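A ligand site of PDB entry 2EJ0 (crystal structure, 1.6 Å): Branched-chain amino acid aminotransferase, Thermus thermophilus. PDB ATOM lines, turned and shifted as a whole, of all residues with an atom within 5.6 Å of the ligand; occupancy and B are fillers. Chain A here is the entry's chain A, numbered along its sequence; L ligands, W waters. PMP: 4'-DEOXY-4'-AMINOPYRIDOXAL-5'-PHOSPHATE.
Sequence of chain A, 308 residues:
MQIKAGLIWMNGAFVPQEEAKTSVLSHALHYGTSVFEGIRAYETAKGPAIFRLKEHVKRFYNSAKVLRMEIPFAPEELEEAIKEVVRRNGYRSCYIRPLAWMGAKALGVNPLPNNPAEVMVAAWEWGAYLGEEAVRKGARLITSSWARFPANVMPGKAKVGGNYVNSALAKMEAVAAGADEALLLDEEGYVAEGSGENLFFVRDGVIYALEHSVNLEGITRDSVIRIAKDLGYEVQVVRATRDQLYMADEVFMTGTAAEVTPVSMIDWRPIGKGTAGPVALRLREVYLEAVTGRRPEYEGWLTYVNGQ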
ATOM      1  N   PHE A  36      21.380  -4.387  -3.890  1.00  0.00           N
ATOM      2  CA  PHE A  36      21.399  -4.109  -5.314  1.00  0.00           C
ATOM      3  C   PHE A  36      20.792  -5.233  -6.110  1.00  0.00           C
ATOM      4  O   PHE A  36      20.432  -6.282  -5.568  1.00  0.00           O
ATOM      5  CB  PHE A  36      22.845  -3.843  -5.779  1.00  0.00           C
ATOM      6  CG  PHE A  36      23.741  -5.058  -5.703  1.00  0.00           C
ATOM      7  CD1 PHE A  36      23.880  -5.906  -6.809  1.00  0.00           C
ATOM      8  CD2 PHE A  36      24.461  -5.341  -4.551  1.00  0.00           C
ATOM      9  CE1 PHE A  36      24.722  -7.018  -6.753  1.00  0.00           C
ATOM     10  CE2 PHE A  36      25.310  -6.452  -4.483  1.00  0.00           C
ATOM     11  CZ  PHE A  36      25.440  -7.290  -5.583  1.00  0.00           C
ATOM     12  N   GLY A  38      20.819  -7.111 -10.330  1.00  0.00           N
ATOM     13  CA  GLY A  38      21.523  -7.269 -11.585  1.00  0.00           C
ATOM     14  C   GLY A  38      20.435  -7.644 -12.569  1.00  0.00           C
ATOM     15  O   GLY A  38      19.842  -8.713 -12.440  1.00  0.00           O
ATOM     16  N   HIS A  56      13.044  -9.313 -10.333  1.00  0.00           N
ATOM     17  CA  HIS A  56      14.222  -8.601  -9.858  1.00  0.00           C
ATOM     18  C   HIS A  56      13.825  -7.460  -8.933  1.00  0.00           C
ATOM     19  O   HIS A  56      14.436  -7.266  -7.886  1.00  0.00           O
ATOM     20  CB  HIS A  56      15.039  -8.076 -11.047  1.00  0.00           C
ATOM     21  CG  HIS A  56      15.902  -9.118 -11.683  1.00  0.00           C
ATOM     22  ND1 HIS A  56      17.076  -9.561 -11.103  1.00  0.00           N
ATOM     23  CD2 HIS A  56      15.746  -9.839 -12.815  1.00  0.00           C
ATOM     24  CE1 HIS A  56      17.598 -10.518 -11.861  1.00  0.00           C
ATOM     25  NE2 HIS A  56      16.805 -10.702 -12.903  1.00  0.00           N
ATOM     26  N   ARG A  59      12.763  -8.846  -5.593  1.00  0.00           N
ATOM     27  CA  ARG A  59      13.905  -9.270  -4.794  1.00  0.00           C
ATOM     28  C   ARG A  59      14.655  -8.063  -4.224  1.00  0.00           C
ATOM     29  O   ARG A  59      15.205  -8.124  -3.123  1.00  0.00           O
ATOM     30  CB  ARG A  59      14.848 -10.143  -5.618  1.00  0.00           C
ATOM     31  CG  ARG A  59      15.929 -10.833  -4.781  1.00  0.00           C
ATOM     32  CD  ARG A  59      16.619 -11.936  -5.557  1.00  0.00           C
ATOM     33  NE  ARG A  59      17.382 -11.418  -6.687  1.00  0.00           N
ATOM     34  CZ  ARG A  59      17.957 -12.176  -7.617  1.00  0.00           C
ATOM     35  NH1 ARG A  59      17.845 -13.504  -7.557  1.00  0.00           N
ATOM     36  NH2 ARG A  59      18.637 -11.613  -8.605  1.00  0.00           N
ATOM     37  N   ARG A 148      30.945 -20.309   1.931  1.00  0.00           N
ATOM     38  CA  ARG A 148      29.794 -19.425   1.766  1.00  0.00           C
ATOM     39  C   ARG A 148      29.231 -19.259   3.167  1.00  0.00           C
ATOM     40  O   ARG A 148      29.142 -20.214   3.928  1.00  0.00           O
ATOM     41  CB  ARG A 148      28.757 -20.079   0.858  1.00  0.00           C
ATOM     42  CG  ARG A 148      27.819 -19.104   0.223  1.00  0.00           C
ATOM     43  CD  ARG A 148      28.629 -18.088  -0.558  1.00  0.00           C
ATOM     44  NE  ARG A 148      27.771 -17.179  -1.300  1.00  0.00           N
ATOM     45  CZ  ARG A 148      28.168 -16.001  -1.753  1.00  0.00           C
ATOM     46  NH1 ARG A 148      29.416 -15.579  -1.555  1.00  0.00           N
ATOM     47  NH2 ARG A 148      27.303 -15.240  -2.418  1.00  0.00           N
ATOM     48  N   LYS A 159      20.681  -9.667  -1.795  1.00  0.00           N
ATOM     49  CA  LYS A 159      21.885  -9.154  -2.425  1.00  0.00           C
ATOM     50  C   LYS A 159      22.307  -7.921  -1.626  1.00  0.00           C
ATOM     51  O   LYS A 159      22.123  -6.780  -2.062  1.00  0.00           O
ATOM     52  CB  LYS A 159      21.621  -8.786  -3.899  1.00  0.00           C
ATOM     53  CG  LYS A 159      21.243  -9.996  -4.744  1.00  0.00           C
ATOM     54  CD  LYS A 159      21.096  -9.647  -6.233  1.00  0.00           C
ATOM     55  CE  LYS A 159      22.453  -9.487  -6.898  1.00  0.00           C
ATOM     56  NZ  LYS A 159      22.318  -9.325  -8.380  1.00  0.00           N
ATOM     57  N   TYR A 164      29.020  -9.549  -0.488  1.00  0.00           N
ATOM     58  CA  TYR A 164      29.986  -9.736  -1.557  1.00  0.00           C
ATOM     59  C   TYR A 164      31.470  -9.663  -1.263  1.00  0.00           C
ATOM     60  O   TYR A 164      32.304  -9.839  -2.149  1.00  0.00           O
ATOM     61  CB  TYR A 164      29.571  -8.857  -2.751  1.00  0.00           C
ATOM     62  CG  TYR A 164      28.247  -9.360  -3.291  1.00  0.00           C
ATOM     63  CD1 TYR A 164      27.051  -9.086  -2.639  1.00  0.00           C
ATOM     64  CD2 TYR A 164      28.215 -10.251  -4.371  1.00  0.00           C
ATOM     65  CE1 TYR A 164      25.848  -9.679  -3.035  1.00  0.00           C
ATOM     66  CE2 TYR A 164      27.019 -10.842  -4.779  1.00  0.00           C
ATOM     67  CZ  TYR A 164      25.843 -10.555  -4.100  1.00  0.00           C
ATOM     68  OH  TYR A 164      24.672 -11.167  -4.482  1.00  0.00           O
ATOM     69  N   SER A 167      32.180 -13.126  -1.703  1.00  0.00           N
ATOM     70  CA  SER A 167      32.259 -13.443  -3.130  1.00  0.00           C
ATOM     71  C   SER A 167      33.558 -12.892  -3.728  1.00  0.00           C
ATOM     72  O   SER A 167      34.201 -13.566  -4.530  1.00  0.00           O
ATOM     73  CB  SER A 167      31.080 -12.835  -3.878  1.00  0.00           C
ATOM     74  OG  SER A 167      29.871 -13.503  -3.541  1.00  0.00           O
ATOM     75  N   GLU A 193      27.503 -22.392  -3.997  1.00  0.00           N
ATOM     76  CA  GLU A 193      27.277 -21.710  -5.271  1.00  0.00           C
ATOM     77  C   GLU A 193      28.587 -21.073  -5.745  1.00  0.00           C
ATOM     78  O   GLU A 193      29.599 -21.141  -5.050  1.00  0.00           O
ATOM     79  CB  GLU A 193      26.198 -20.633  -5.102  1.00  0.00           C
ATOM     80  CG  GLU A 193      26.624 -19.414  -4.271  1.00  0.00           C
ATOM     81  CD  GLU A 193      25.482 -18.442  -3.950  1.00  0.00           C
ATOM     82  OE1 GLU A 193      24.521 -18.352  -4.736  1.00  0.00           O
ATOM     83  OE2 GLU A 193      25.556 -17.758  -2.907  1.00  0.00           O
ATOM     84  N   GLY A 194      28.567 -20.485  -6.936  1.00  0.00           N
ATOM     85  CA  GLY A 194      29.745 -19.803  -7.447  1.00  0.00           C
ATOM     86  C   GLY A 194      29.764 -18.422  -6.799  1.00  0.00           C
ATOM     87  O   GLY A 194      28.824 -18.081  -6.077  1.00  0.00           O
ATOM     88  N   SER A 195      30.795 -17.628  -7.036  1.00  0.00           N
ATOM     89  CA  SER A 195      30.844 -16.304  -6.422  1.00  0.00           C
ATOM     90  C   SER A 195      29.628 -15.460  -6.812  1.00  0.00           C
ATOM     91  O   SER A 195      29.229 -14.550  -6.088  1.00  0.00           O
ATOM     92  CB  SER A 195      32.132 -15.567  -6.795  1.00  0.00           C
ATOM     93  OG  SER A 195      32.121 -15.141  -8.145  1.00  0.00           O
ATOM     94  N   GLY A 196      29.035 -15.779  -7.958  1.00  0.00           N
ATOM     95  CA  GLY A 196      27.872 -15.044  -8.420  1.00  0.00           C
ATOM     96  C   GLY A 196      26.969 -15.851  -9.332  1.00  0.00           C
ATOM     97  O   GLY A 196      26.263 -15.291 -10.158  1.00  0.00           O
ATOM     98  N   GLU A 197      26.983 -17.177  -9.158  1.00  0.00           N
ATOM     99  CA  GLU A 197      26.168 -18.057  -9.997  1.00  0.00           C
ATOM    100  C   GLU A 197      25.639 -19.248  -9.220  1.00  0.00           C
ATOM    101  O   GLU A 197      26.255 -19.669  -8.249  1.00  0.00           O
ATOM    102  CB  GLU A 197      26.994 -18.613 -11.159  1.00  0.00           C
ATOM    103  CG  GLU A 197      27.765 -17.594 -11.992  1.00  0.00           C
ATOM    104  CD  GLU A 197      29.156 -17.310 -11.446  1.00  0.00           C
ATOM    105  OE1 GLU A 197      29.941 -16.678 -12.175  1.00  0.00           O
ATOM    106  OE2 GLU A 197      29.457 -17.705 -10.303  1.00  0.00           O
ATOM    107  N   ASN A 198      24.506 -19.790  -9.653  1.00  0.00           N
ATOM    108  CA  ASN A 198      23.951 -20.980  -9.018  1.00  0.00           C
ATOM    109  C   ASN A 198      24.456 -22.178  -9.808  1.00  0.00           C
ATOM    110  O   ASN A 198      24.796 -22.046 -10.994  1.00  0.00           O
ATOM    111  CB  ASN A 198      22.418 -20.965  -9.041  1.00  0.00           C
ATOM    112  CG  ASN A 198      21.835 -19.914  -8.122  1.00  0.00           C
ATOM    113  OD1 ASN A 198      20.994 -19.116  -8.528  1.00  0.00           O
ATOM    114  ND2 ASN A 198      22.266 -19.914  -6.855  1.00  0.00           N
ATOM    115  N   LEU A 216      21.741 -17.659  -3.070  1.00  0.00           N
ATOM    116  CA  LEU A 216      20.735 -16.710  -3.520  1.00  0.00           C
ATOM    117  C   LEU A 216      19.776 -17.549  -4.370  1.00  0.00           C
ATOM    118  O   LEU A 216      20.197 -18.488  -5.040  1.00  0.00           O
ATOM    119  CB  LEU A 216      21.367 -15.639  -4.416  1.00  0.00           C
ATOM    120  CG  LEU A 216      20.486 -14.445  -4.793  1.00  0.00           C
ATOM    121  CD1 LEU A 216      20.319 -13.545  -3.580  1.00  0.00           C
ATOM    122  CD2 LEU A 216      21.115 -13.662  -5.939  1.00  0.00           C
ATOM    123  N   GLU A 217      18.481 -17.235  -4.309  1.00  0.00           N
ATOM    124  CA  GLU A 217      17.495 -17.959  -5.114  1.00  0.00           C
ATOM    125  C   GLU A 217      17.541 -17.333  -6.498  1.00  0.00           C
ATOM    126  O   GLU A 217      16.813 -16.384  -6.788  1.00  0.00           O
ATOM    127  CB  GLU A 217      16.103 -17.803  -4.511  1.00  0.00           C
ATOM    128  CG  GLU A 217      15.938 -18.454  -3.143  1.00  0.00           C
ATOM    129  CD  GLU A 217      14.599 -18.150  -2.521  1.00  0.00           C
ATOM    130  OE1 GLU A 217      14.195 -18.862  -1.577  1.00  0.00           O
ATOM    131  OE2 GLU A 217      13.940 -17.171  -2.963  1.00  0.00           O
ATOM    132  N   GLY A 218      18.410 -17.870  -7.353  1.00  0.00           N
ATOM    133  CA  GLY A 218      18.564 -17.318  -8.686  1.00  0.00           C
ATOM    134  C   GLY A 218      17.347 -17.309  -9.593  1.00  0.00           C
ATOM    135  O   GLY A 218      16.585 -18.268  -9.669  1.00  0.00           O
ATOM    136  N   ILE A 219      17.172 -16.187 -10.285  1.00  0.00           N
ATOM    137  CA  ILE A 219      16.073 -16.034 -11.212  1.00  0.00           C
ATOM    138  C   ILE A 219      16.447 -16.781 -12.501  1.00  0.00           C
ATOM    139  O   ILE A 219      15.577 -17.281 -13.209  1.00  0.00           O
ATOM    140  CB  ILE A 219      15.804 -14.543 -11.489  1.00  0.00           C
ATOM    141  CG1 ILE A 219      15.191 -13.911 -10.229  1.00  0.00           C
ATOM    142  CG2 ILE A 219      14.874 -14.381 -12.689  1.00  0.00           C
ATOM    143  CD1 ILE A 219      15.091 -12.393 -10.255  1.00  0.00           C
ATOM    144  N   THR A 220      17.746 -16.871 -12.788  1.00  0.00           N
ATOM    145  CA  THR A 220      18.185 -17.603 -13.977  1.00  0.00           C
ATOM    146  C   THR A 220      18.016 -19.088 -13.675  1.00  0.00           C
ATOM    147  O   THR A 220      17.590 -19.864 -14.537  1.00  0.00           O
ATOM    148  CB  THR A 220      19.659 -17.306 -14.319  1.00  0.00           C
ATOM    149  OG1 THR A 220      19.887 -15.888 -14.296  1.00  0.00           O
ATOM    150  CG2 THR A 220      19.983 -17.830 -15.709  1.00  0.00           C
ATOM    151  N   ARG A 221      18.333 -19.481 -12.451  1.00  0.00           N
ATOM    152  CA  ARG A 221      18.179 -20.863 -12.011  1.00  0.00           C
ATOM    153  C   ARG A 221      16.711 -21.253 -12.197  1.00  0.00           C
ATOM    154  O   ARG A 221      16.396 -22.311 -12.743  1.00  0.00           O
ATOM    155  CB  ARG A 221      18.582 -20.996 -10.540  1.00  0.00           C
ATOM    156  CG  ARG A 221      18.241 -22.338  -9.892  1.00  0.00           C
ATOM    157  CD  ARG A 221      18.581 -22.317  -8.411  1.00  0.00           C
ATOM    158  NE  ARG A 221      18.309 -23.596  -7.750  1.00  0.00           N
ATOM    159  CZ  ARG A 221      17.102 -24.023  -7.405  1.00  0.00           C
ATOM    160  NH1 ARG A 221      16.030 -23.277  -7.657  1.00  0.00           N
ATOM    161  NH2 ARG A 221      16.962 -25.204  -6.805  1.00  0.00           N
ATOM    162  N   THR A 254      24.383 -20.839 -13.620  1.00  0.00           N
ATOM    163  CA  THR A 254      23.365 -19.907 -14.094  1.00  0.00           C
ATOM    164  C   THR A 254      23.450 -18.596 -13.319  1.00  0.00           C
ATOM    165  O   THR A 254      23.782 -18.584 -12.125  1.00  0.00           O
ATOM    166  CB  THR A 254      21.938 -20.469 -13.941  1.00  0.00           C
ATOM    167  OG1 THR A 254      21.669 -20.722 -12.562  1.00  0.00           O
ATOM    168  CG2 THR A 254      21.774 -21.745 -14.743  1.00  0.00           C
ATOM    169  N   GLY A 255      23.158 -17.505 -14.013  1.00  0.00           N
ATOM    170  CA  GLY A 255      23.195 -16.196 -13.391  1.00  0.00           C
ATOM    171  C   GLY A 255      22.774 -15.172 -14.427  1.00  0.00           C
ATOM    172  O   GLY A 255      22.820 -15.460 -15.617  1.00  0.00           O
ATOM    173  N   THR A 256      22.368 -13.989 -13.982  1.00  0.00           N
ATOM    174  CA  THR A 256      21.944 -12.977 -14.942  1.00  0.00           C
ATOM    175  C   THR A 256      23.084 -12.614 -15.894  1.00  0.00           C
ATOM    176  O   THR A 256      22.864 -12.488 -17.104  1.00  0.00           O
ATOM    177  CB  THR A 256      21.448 -11.721 -14.209  1.00  0.00           C
ATOM    178  OG1 THR A 256      20.259 -12.051 -13.477  1.00  0.00           O
ATOM    179  CG2 THR A 256      21.130 -10.618 -15.204  1.00  0.00           C
ATOM    180  N   ALA A 257      24.285 -12.479 -15.366  1.00  0.00           N
ATOM    181  CA  ALA A 257      25.433 -12.136 -16.189  1.00  0.00           C
ATOM    182  C   ALA A 257      25.982 -13.368 -16.898  1.00  0.00           C
ATOM    183  O   ALA A 257      26.343 -13.315 -18.070  1.00  0.00           O
ATOM    184  CB  ALA A 257      26.526 -11.491 -15.342  1.00  0.00           C
HETATM  185  N1  PMP L   1      24.272 -16.145  -6.476  1.00  0.00           N
HETATM  186  C2  PMP L   1      24.780 -14.918  -6.181  1.00  0.00           C
HETATM  187  C2A PMP L   1      25.527 -14.755  -4.885  1.00  0.00           C
HETATM  188  C3  PMP L   1      24.601 -13.853  -7.062  1.00  0.00           C
HETATM  189  O3  PMP L   1      25.061 -12.595  -6.729  1.00  0.00           O
HETATM  190  C4  PMP L   1      23.906 -14.051  -8.240  1.00  0.00           C
HETATM  191  C4A PMP L   1      23.846 -12.875  -9.307  1.00  0.00           C
HETATM  192  N4A PMP L   1      24.983 -12.796 -10.090  1.00  0.00           N
HETATM  193  C5  PMP L   1      23.381 -15.331  -8.505  1.00  0.00           C
HETATM  194  C6  PMP L   1      23.579 -16.346  -7.630  1.00  0.00           C
HETATM  195  C5A PMP L   1      22.486 -15.620  -9.714  1.00  0.00           C
HETATM  196  O4P PMP L   1      21.201 -15.042  -9.484  1.00  0.00           O
HETATM  197  P   PMP L   1      20.362 -14.557 -10.776  1.00  0.00           P
HETATM  198  O1P PMP L   1      21.089 -13.400 -11.368  1.00  0.00           O
HETATM  199  O2P PMP L   1      19.005 -14.060 -10.106  1.00  0.00           O
HETATM  200  O3P PMP L   1      20.101 -15.740 -11.629  1.00  0.00           O
HETATM  201  O   HOH W   1      26.925 -11.446  -8.578  1.00  0.00           O
HETATM  202  O   HOH W   2      20.702 -18.341 -11.075  1.00  0.00           O
HETATM  203  O   HOH W   3      20.654 -10.713 -10.609  1.00  0.00           O
HETATM  204  O   HOH W   4      24.225 -10.211 -11.998  1.00  0.00           O
HETATM  205  O   HOH W   5      25.135  -9.478  -9.117  1.00  0.00           O
HETATM  206  O   HOH W   6      25.899 -14.131 -13.055  1.00  0.00           O
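A nitrogen (N1) of the ligand sits at hydrogen-bond distance from the side-chain carboxylate of Glu 193 (2.8 Å). OH of Tyr 164 sits at hydrogen-bond distance from O3 of the ligand (2.7 Å). The side-chain hydroxyl of Thr 220 lies within hydrogen-bond range of an oxygen (O3P) of the ligand (2.7 Å). O2P of the ligand is in salt-bridge range of NH1 of Arg 59 (2.9 Å). An oxygen (O3P) of the ligand sits at hydrogen-bond distance from the backbone NH of Thr 220 (2.9 Å). O2P of the ligand lies within hydrogen-bond range of N of Ile 219, 2.8 Å away. The side-chain hydroxyl of Thr 256 lies within hydrogen-bond range of an oxygen (O1P) of the ligand (2.6 Å). N of Thr 256 sits at hydrogen-bond distance from O1P of the ligand (3.0 Å). N4A of the ligand sits at hydrogen-bond distance from O of Gly 196, at 2.8 Å.
The backbone carbonyl oxygen (O) of Glu 217 lies within hydrogen-bond range of the guanidinium group (NH1) of Arg 59 (3.2 Å). The backbone NH (N) of Asn 198 is in hydrogen-bond range of the backbone carbonyl oxygen (O) of Thr 254, at 2.8 Å. O of Ser 195 lies within hydrogen-bond range of OG of Ser 167 (2.8 Å). The backbone carbonyl oxygen of Gly 255 sits close to the side-chain hydroxyl of Thr 220 (3.2 Å). The backbone carbonyl oxygen of Lys 159 lies within hydrogen-bond range of the backbone NH of Phe 36 (3.1 Å). The side-chain carboxylate of Glu 193 lies within hydrogen-bond range of the backbone NH of Leu 216 (3.3 Å). The side-chain hydroxyl (OG1) of Thr 220 is in hydrogen-bond range of the backbone NH (N) of Thr 256. The side-chain carboxylate (OE2) of Glu 193 is in salt-bridge range of the guanidinium group (NE) of Arg 148.
Merely in contact with the ligand: Arg 148, Gly 218, Gly 255, Leu 216, Glu 197, Asn 198, Ser 195 and Lys 159. Of the 24 residues printed, 15 come within 4 Å of the ligand. The nearest printed residue that does not touch the ligand is Thr 254 (4.03 Å).
Water W2 lies within hydrogen-bond range of OD1 of Asn 198 (2.7 Å), O3P of the ligand (2.7 Å), N of Arg 221 (3.0 Å) and OG1 of Thr 254 (3.0 Å). Water W3 lies within hydrogen-bond range of O1P of the ligand (2.8 Å), O of Gly 38 (2.8 Å), NH2 of Arg 59 (3.0 Å), NZ of Lys 159 (3.1 Å) and OG1 of Thr 256 (3.2 Å). Water W6 lies within hydrogen-bond range of O of Gly 196 (3.1 Å), N of Ala 257 (3.3 Å) and N4A of the ligand (3.4 Å). Water W5 bridges the side-chain amino group of Lys 159 (2.9 Å) and a nitrogen (N4A) of the ligand (3.5 Å).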
